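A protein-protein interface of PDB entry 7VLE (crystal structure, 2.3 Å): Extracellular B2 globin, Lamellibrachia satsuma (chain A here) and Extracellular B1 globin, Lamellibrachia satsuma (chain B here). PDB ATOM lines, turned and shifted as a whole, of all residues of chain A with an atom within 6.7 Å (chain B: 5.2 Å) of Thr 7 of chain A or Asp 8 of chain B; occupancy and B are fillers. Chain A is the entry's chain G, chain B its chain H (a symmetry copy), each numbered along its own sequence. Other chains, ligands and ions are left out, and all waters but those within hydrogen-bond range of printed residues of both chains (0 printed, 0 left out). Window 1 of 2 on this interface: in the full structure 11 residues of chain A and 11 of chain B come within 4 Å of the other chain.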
ATOM      1  N   SER A   4     -20.614   4.745 -23.855  1.00  0.00           N
ATOM      2  CA  SER A   4     -21.595   3.858 -24.461  1.00  0.00           C
ATOM      3  C   SER A   4     -22.448   3.192 -23.391  1.00  0.00           C
ATOM      4  O   SER A   4     -21.957   2.824 -22.320  1.00  0.00           O
ATOM      5  CB  SER A   4     -20.891   2.795 -25.304  1.00  0.00           C
ATOM      6  OG  SER A   4     -20.197   3.381 -26.392  1.00  0.00           O
ATOM      7  N   CYS A   5     -23.737   3.037 -23.683  1.00  0.00           N
ATOM      8  CA  CYS A   5     -24.646   2.303 -22.805  1.00  0.00           C
ATOM      9  C   CYS A   5     -24.360   0.815 -22.978  1.00  0.00           C
ATOM     10  O   CYS A   5     -24.778   0.196 -23.960  1.00  0.00           O
ATOM     11  CB  CYS A   5     -26.097   2.656 -23.119  1.00  0.00           C
ATOM     12  SG  CYS A   5     -27.382   1.639 -22.319  1.00  0.00           S
ATOM     13  N   THR A   6     -23.631   0.238 -22.023  1.00  0.00           N
ATOM     14  CA  THR A   6     -23.214  -1.153 -22.105  1.00  0.00           C
ATOM     15  C   THR A   6     -24.318  -2.080 -21.596  1.00  0.00           C
ATOM     16  O   THR A   6     -25.337  -1.644 -21.052  1.00  0.00           O
ATOM     17  CB  THR A   6     -21.927  -1.380 -21.309  1.00  0.00           C
ATOM     18  OG1 THR A   6     -22.182  -1.195 -19.910  1.00  0.00           O
ATOM     19  CG2 THR A   6     -20.839  -0.409 -21.753  1.00  0.00           C
ATOM     20  N   THR A   7     -24.099  -3.386 -21.784  1.00  0.00           N
ATOM     21  CA  THR A   7     -25.064  -4.386 -21.332  1.00  0.00           C
ATOM     22  C   THR A   7     -25.261  -4.318 -19.821  1.00  0.00           C
ATOM     23  O   THR A   7     -26.395  -4.356 -19.326  1.00  0.00           O
ATOM     24  CB  THR A   7     -24.597  -5.785 -21.742  1.00  0.00           C
ATOM     25  OG1 THR A   7     -24.590  -5.901 -23.171  1.00  0.00           O
ATOM     26  CG2 THR A   7     -25.507  -6.854 -21.149  1.00  0.00           C
ATOM     27  N   GLU A   8     -24.152  -4.240 -19.075  1.00  0.00           N
ATOM     28  CA  GLU A   8     -24.191  -4.080 -17.620  1.00  0.00           C
ATOM     29  C   GLU A   8     -24.988  -2.860 -17.222  1.00  0.00           C
ATOM     30  O   GLU A   8     -25.761  -2.886 -16.257  1.00  0.00           O
ATOM     31  CB  GLU A   8     -22.783  -3.898 -17.064  1.00  0.00           C
ATOM     32  CG  GLU A   8     -21.836  -5.006 -17.311  1.00  0.00           C
ATOM     33  CD  GLU A   8     -21.169  -4.920 -18.659  1.00  0.00           C
ATOM     34  OE1 GLU A   8     -21.536  -4.052 -19.482  1.00  0.00           O
ATOM     35  OE2 GLU A   8     -20.263  -5.740 -18.889  1.00  0.00           O
ATOM     36  N   ASP A   9     -24.705  -1.747 -17.890  1.00  0.00           N
ATOM     37  CA  ASP A   9     -25.376  -0.499 -17.582  1.00  0.00           C
ATOM     38  C   ASP A   9     -26.878  -0.644 -17.753  1.00  0.00           C
ATOM     39  O   ASP A   9     -27.655  -0.141 -16.933  1.00  0.00           O
ATOM     40  CB  ASP A   9     -24.815   0.607 -18.475  1.00  0.00           C
ATOM     41  CG  ASP A   9     -23.423   1.045 -18.050  1.00  0.00           C
ATOM     42  OD1 ASP A   9     -23.070   0.827 -16.872  1.00  0.00           O
ATOM     43  OD2 ASP A   9     -22.692   1.618 -18.885  1.00  0.00           O
ATOM     44  N   ARG A  10     -27.301  -1.374 -18.787  1.00  0.00           N
ATOM     45  CA  ARG A  10     -28.724  -1.553 -19.055  1.00  0.00           C
ATOM     46  C   ARG A  10     -29.410  -2.308 -17.923  1.00  0.00           C
ATOM     47  O   ARG A  10     -30.459  -1.882 -17.427  1.00  0.00           O
ATOM     48  CB  ARG A  10     -28.912  -2.283 -20.386  1.00  0.00           C
ATOM     49  CG  ARG A  10     -28.659  -1.408 -21.595  1.00  0.00           C
ATOM     50  CD  ARG A  10     -28.008  -2.169 -22.739  1.00  0.00           C
ATOM     51  NE  ARG A  10     -27.259  -1.274 -23.617  1.00  0.00           N
ATOM     52  CZ  ARG A  10     -27.692  -0.839 -24.797  1.00  0.00           C
ATOM     53  NH1 ARG A  10     -28.873  -1.226 -25.256  1.00  0.00           N
ATOM     54  NH2 ARG A  10     -26.938  -0.021 -25.521  1.00  0.00           N
ATOM     55  N   ARG A  11     -28.834  -3.444 -17.513  1.00  0.00           N
ATOM     56  CA  ARG A  11     -29.369  -4.190 -16.378  1.00  0.00           C
ATOM     57  C   ARG A  11     -29.474  -3.310 -15.142  1.00  0.00           C
ATOM     58  O   ARG A  11     -30.446  -3.396 -14.383  1.00  0.00           O
ATOM     59  CB  ARG A  11     -28.479  -5.396 -16.078  1.00  0.00           C
ATOM     60  CG  ARG A  11     -28.327  -6.384 -17.214  1.00  0.00           C
ATOM     61  CD  ARG A  11     -27.085  -7.231 -17.004  1.00  0.00           C
ATOM     62  NE  ARG A  11     -27.007  -8.348 -17.939  1.00  0.00           N
ATOM     63  CZ  ARG A  11     -25.913  -9.078 -18.135  1.00  0.00           C
ATOM     64  NH1 ARG A  11     -24.802  -8.800 -17.468  1.00  0.00           N
ATOM     65  NH2 ARG A  11     -25.929 -10.080 -19.003  1.00  0.00           N
ATOM     66  N   GLU A  12     -28.471  -2.459 -14.928  1.00  0.00           N
ATOM     67  CA  GLU A  12     -28.456  -1.586 -13.761  1.00  0.00           C
ATOM     68  C   GLU A  12     -29.547  -0.527 -13.848  1.00  0.00           C
ATOM     69  O   GLU A  12     -30.194  -0.210 -12.842  1.00  0.00           O
ATOM     70  CB  GLU A  12     -27.079  -0.940 -13.628  1.00  0.00           C
ATOM     71  CG  GLU A  12     -26.873  -0.144 -12.360  1.00  0.00           C
ATOM     72  CD  GLU A  12     -25.404   0.059 -12.046  1.00  0.00           C
ATOM     73  OE1 GLU A  12     -25.099   0.736 -11.044  1.00  0.00           O
ATOM     74  OE2 GLU A  12     -24.556  -0.465 -12.798  1.00  0.00           O
ATOM     75  N   GLN A  14     -32.343  -0.858 -15.516  1.00  0.00           N
ATOM     76  CA  GLN A  14     -33.621  -1.543 -15.376  1.00  0.00           C
ATOM     77  C   GLN A  14     -33.950  -1.814 -13.914  1.00  0.00           C
ATOM     78  O   GLN A  14     -35.125  -1.793 -13.532  1.00  0.00           O
ATOM     79  CB  GLN A  14     -33.608  -2.839 -16.192  1.00  0.00           C
ATOM     80  CG  GLN A  14     -33.809  -2.608 -17.688  1.00  0.00           C
ATOM     81  CD  GLN A  14     -33.474  -3.821 -18.540  1.00  0.00           C
ATOM     82  OE1 GLN A  14     -32.931  -4.812 -18.049  1.00  0.00           O
ATOM     83  NE2 GLN A  14     -33.794  -3.744 -19.827  1.00  0.00           N
ATOM     84  N   CYS A 136     -27.229   5.345 -20.468  1.00  0.00           N
ATOM     85  CA  CYS A 136     -28.326   4.672 -21.148  1.00  0.00           C
ATOM     86  C   CYS A 136     -29.512   5.587 -21.394  1.00  0.00           C
ATOM     87  O   CYS A 136     -30.241   5.393 -22.373  1.00  0.00           O
ATOM     88  CB  CYS A 136     -28.757   3.448 -20.344  1.00  0.00           C
ATOM     89  SG  CYS A 136     -27.477   2.190 -20.360  1.00  0.00           S
ATOM     90  N   CYS B   4     -14.473  -3.204 -25.587  1.00  0.00           N
ATOM     91  CA  CYS B   4     -15.839  -3.166 -25.080  1.00  0.00           C
ATOM     92  C   CYS B   4     -15.927  -4.004 -23.811  1.00  0.00           C
ATOM     93  O   CYS B   4     -15.039  -4.803 -23.502  1.00  0.00           O
ATOM     94  CB  CYS B   4     -16.856  -3.648 -26.131  1.00  0.00           C
ATOM     95  SG  CYS B   4     -16.661  -5.367 -26.696  1.00  0.00           S
ATOM     96  N   SER B   5     -17.023  -3.814 -23.075  1.00  0.00           N
ATOM     97  CA  SER B   5     -17.203  -4.447 -21.777  1.00  0.00           C
ATOM     98  C   SER B   5     -17.309  -5.966 -21.910  1.00  0.00           C
ATOM     99  O   SER B   5     -17.541  -6.513 -22.992  1.00  0.00           O
ATOM    100  CB  SER B   5     -18.453  -3.905 -21.086  1.00  0.00           C
ATOM    101  OG  SER B   5     -19.628  -4.340 -21.751  1.00  0.00           O
ATOM    102  N   GLU B   6     -17.146  -6.646 -20.771  1.00  0.00           N
ATOM    103  CA  GLU B   6     -17.191  -8.106 -20.756  1.00  0.00           C
ATOM    104  C   GLU B   6     -18.564  -8.631 -21.156  1.00  0.00           C
ATOM    105  O   GLU B   6     -18.671  -9.668 -21.819  1.00  0.00           O
ATOM    106  CB  GLU B   6     -16.800  -8.632 -19.373  1.00  0.00           C
ATOM    107  CG  GLU B   6     -16.916 -10.142 -19.226  1.00  0.00           C
ATOM    108  CD  GLU B   6     -16.469 -10.634 -17.864  1.00  0.00           C
ATOM    109  OE1 GLU B   6     -15.261 -10.535 -17.561  1.00  0.00           O
ATOM    110  OE2 GLU B   6     -17.327 -11.114 -17.094  1.00  0.00           O
ATOM    111  N   ALA B   7     -19.632  -7.933 -20.757  1.00  0.00           N
ATOM    112  CA  ALA B   7     -20.972  -8.393 -21.109  1.00  0.00           C
ATOM    113  C   ALA B   7     -21.330  -8.069 -22.552  1.00  0.00           C
ATOM    114  O   ALA B   7     -22.056  -8.842 -23.188  1.00  0.00           O
ATOM    115  CB  ALA B   7     -22.017  -7.792 -20.171  1.00  0.00           C
ATOM    116  N   ASP B   8     -20.854  -6.938 -23.077  1.00  0.00           N
ATOM    117  CA  ASP B   8     -21.045  -6.646 -24.495  1.00  0.00           C
ATOM    118  C   ASP B   8     -20.308  -7.662 -25.356  1.00  0.00           C
ATOM    119  O   ASP B   8     -20.882  -8.245 -26.285  1.00  0.00           O
ATOM    120  CB  ASP B   8     -20.558  -5.235 -24.826  1.00  0.00           C
ATOM    121  CG  ASP B   8     -21.566  -4.166 -24.463  1.00  0.00           C
ATOM    122  OD1 ASP B   8     -21.182  -2.978 -24.427  1.00  0.00           O
ATOM    123  OD2 ASP B   8     -22.737  -4.512 -24.206  1.00  0.00           O
ATOM    124  N   ALA B   9     -19.025  -7.881 -25.056  1.00  0.00           N
ATOM    125  CA  ALA B   9     -18.219  -8.822 -25.824  1.00  0.00           C
ATOM    126  C   ALA B   9     -18.783 -10.234 -25.744  1.00  0.00           C
ATOM    127  O   ALA B   9     -18.748 -10.978 -26.730  1.00  0.00           O
ATOM    128  CB  ALA B   9     -16.775  -8.792 -25.326  1.00  0.00           C
ATOM    129  N   THR B  10     -19.306 -10.619 -24.576  1.00  0.00           N
ATOM    130  CA  THR B  10     -19.879 -11.952 -24.417  1.00  0.00           C
ATOM    131  C   THR B  10     -21.040 -12.173 -25.378  1.00  0.00           C
ATOM    132  O   THR B  10     -21.168 -13.248 -25.974  1.00  0.00           O
ATOM    133  CB  THR B  10     -20.343 -12.156 -22.972  1.00  0.00           C
ATOM    134  OG1 THR B  10     -19.225 -12.030 -22.083  1.00  0.00           O
ATOM    135  CG2 THR B  10     -20.976 -13.529 -22.796  1.00  0.00           C
ATOM    136  N   ILE B  11     -21.895 -11.162 -25.538  1.00  0.00           N
ATOM    137  CA  ILE B  11     -23.014 -11.265 -26.471  1.00  0.00           C
ATOM    138  C   ILE B  11     -22.504 -11.375 -27.902  1.00  0.00           C
ATOM    139  O   ILE B  11     -22.951 -12.230 -28.675  1.00  0.00           O
ATOM    140  CB  ILE B  11     -23.958 -10.059 -26.307  1.00  0.00           C
ATOM    141  CG1 ILE B  11     -24.589 -10.046 -24.914  1.00  0.00           C
ATOM    142  CG2 ILE B  11     -25.023 -10.066 -27.390  1.00  0.00           C
ATOM    143  CD1 ILE B  11     -25.504  -8.860 -24.678  1.00  0.00           C
ATOM    144  N   VAL B  12     -21.561 -10.504 -28.274  1.00  0.00           N
ATOM    145  CA  VAL B  12     -21.013 -10.503 -29.627  1.00  0.00           C
ATOM    146  C   VAL B  12     -20.330 -11.829 -29.933  1.00  0.00           C
ATOM    147  O   VAL B  12     -20.500 -12.397 -31.020  1.00  0.00           O
ATOM    148  CB  VAL B  12     -20.044  -9.319 -29.804  1.00  0.00           C
ATOM    149  CG1 VAL B  12     -19.356  -9.385 -31.159  1.00  0.00           C
ATOM    150  CG2 VAL B  12     -20.778  -7.998 -29.630  1.00  0.00           C
ATOM    151  N   ILE B  13     -19.536 -12.336 -28.985  1.00  0.00           N
ATOM    152  CA  ILE B  13     -18.854 -13.614 -29.178  1.00  0.00           C
ATOM    153  C   ILE B  13     -19.866 -14.735 -29.364  1.00  0.00           C
ATOM    154  O   ILE B  13     -19.709 -15.596 -30.239  1.00  0.00           O
ATOM    155  CB  ILE B  13     -17.915 -13.904 -27.991  1.00  0.00           C
ATOM    156  CG1 ILE B  13     -16.707 -12.962 -28.002  1.00  0.00           C
ATOM    157  CG2 ILE B  13     -17.457 -15.354 -28.011  1.00  0.00           C
ATOM    158  CD1 ILE B  13     -15.792 -13.142 -26.804  1.00  0.00           C
ATOM    159  N   ALA B 132     -24.638  -3.954 -28.738  1.00  0.00           N
ATOM    160  CA  ALA B 132     -23.406  -4.576 -28.264  1.00  0.00           C
ATOM    161  C   ALA B 132     -22.398  -4.734 -29.396  1.00  0.00           C
ATOM    162  O   ALA B 132     -21.193  -4.539 -29.196  1.00  0.00           O
ATOM    163  CB  ALA B 132     -23.716  -5.928 -27.625  1.00  0.00           C
ATOM    164  N   ASN B 135     -20.812  -1.460 -30.074  1.00  0.00           N
ATOM    165  CA  ASN B 135     -19.857  -1.151 -29.016  1.00  0.00           C
ATOM    166  C   ASN B 135     -18.551  -1.916 -29.177  1.00  0.00           C
ATOM    167  O   ASN B 135     -17.497  -1.427 -28.760  1.00  0.00           O
ATOM    168  CB  ASN B 135     -20.467  -1.463 -27.648  1.00  0.00           C
ATOM    169  CG  ASN B 135     -21.641  -0.570 -27.313  1.00  0.00           C
ATOM    170  OD1 ASN B 135     -21.838   0.476 -27.932  1.00  0.00           O
ATOM    171  ND2 ASN B 135     -22.423  -0.972 -26.318  1.00  0.00           N
ATOM    172  N   CYS B 136     -18.599  -3.117 -29.753  1.00  0.00           N
ATOM    173  CA  CYS B 136     -17.405  -3.939 -29.899  1.00  0.00           C
ATOM    174  C   CYS B 136     -16.772  -3.844 -31.281  1.00  0.00           C
ATOM    175  O   CYS B 136     -15.543  -3.903 -31.391  1.00  0.00           O
ATOM    176  CB  CYS B 136     -17.727  -5.407 -29.587  1.00  0.00           C
ATOM    177  SG  CYS B 136     -18.280  -5.731 -27.879  1.00  0.00           S
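The side-chain carboxylate of Asp 8 of chain B lies within hydrogen-bond range of the side-chain hydroxyl of Thr 7 of chain A (2.5 Å).
OG of Ser 5 of chain B is in hydrogen-bond range of OE1 of Glu 8 of chain A (3.0 Å).
The backbone NH of Ala 7 of chain B is in hydrogen-bond range of the side-chain carboxylate of Glu 8 of chain A, at 2.9 Å.
Of chain B, only Ala 7, Asp 8 and Ile 11 come within 4 Å of Thr 7 of chain A.
Of chain A, only Thr 6 (3.6 Å) and Thr 7 (2.5 Å) come within 4 Å of Asp 8 of chain B.
Of the printed residues of chain A, Ile 11 of chain B touches Thr 7.
Of the printed residues of chain A, Asn 135 of chain B touches Ser 4 (3.6 Å) and Cys 5 (3.5 Å).
Of the printed residues of chain A, Ser 5 of chain B touches Thr 6 and Glu 8.
Printed residues of chain A within 4 Å of Glu 6 of chain B: Glu 8.
Glu 12 of chain A touches none of the printed residues of chain B.
The nearest residue of chain A that does not touch Asp 8 of chain B is Glu 8 of chain A (4.4 Å).
The side-chain carboxylate (OD1) of Asp 8 of chain B lies within hydrogen-bond range of the side-chain amide nitrogen (ND2) of Asn 135 of chain B, at 3.0 Å.
OG1 of Thr 6 of chain A lies within hydrogen-bond range of OD2 of Asp 9 of chain A (3.0 Å).
SG of Cys 4 of chain B forms a disulfide with SG of Cys 136 of chain B, at 2.0 Å.
The side-chain sulfur (SG) of Cys 5 of chain A forms a disulfide with the side-chain sulfur (SG) of Cys 136 of chain A (2.0 Å).
NE of Arg 10 of chain A sits close to O of Thr 6 of chain A (3.2 Å).
The side-chain hydroxyl (OG1) of Thr 6 of chain A lies within hydrogen-bond range of the side-chain carboxylate (OE1) of Glu 8 of chain A (3.0 Å).
Along chain A the printed residues that touch a printed residue of chain B span positions 4 to 8.
Printed residues of chain B that touch a printed residue of chain A: Ser 5, Glu 6, Ala 7, Asp 8, Ile 11 and Asn 135.
Among the printed residues, 10 pairs touch across the chains.
Among the printed residues, no Asp or Glu carboxylate lies within 4 Å of a Lys or Arg side-chain nitrogen of the other chain.
Ser 4 of chain A touches Asn 135 of chain B (CB to OD1, 3.6 Å).
Cys 5 of chain A touches Asn 135 of chain B (O to ND2, 3.5 Å).
OG of Ser 5 of chain B touches CB of Thr 6 of chain A, at 3.8 Å.
Thr 6 of chain A touches Asp 8 of chain B.
Ala 7 of chain B touches Thr 7 of chain A.
Thr 7 of chain A touches Ile 11 of chain B (OG1 to CD1, 3.4 Å).
Glu 8 of chain A touches Glu 6 of chain B.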
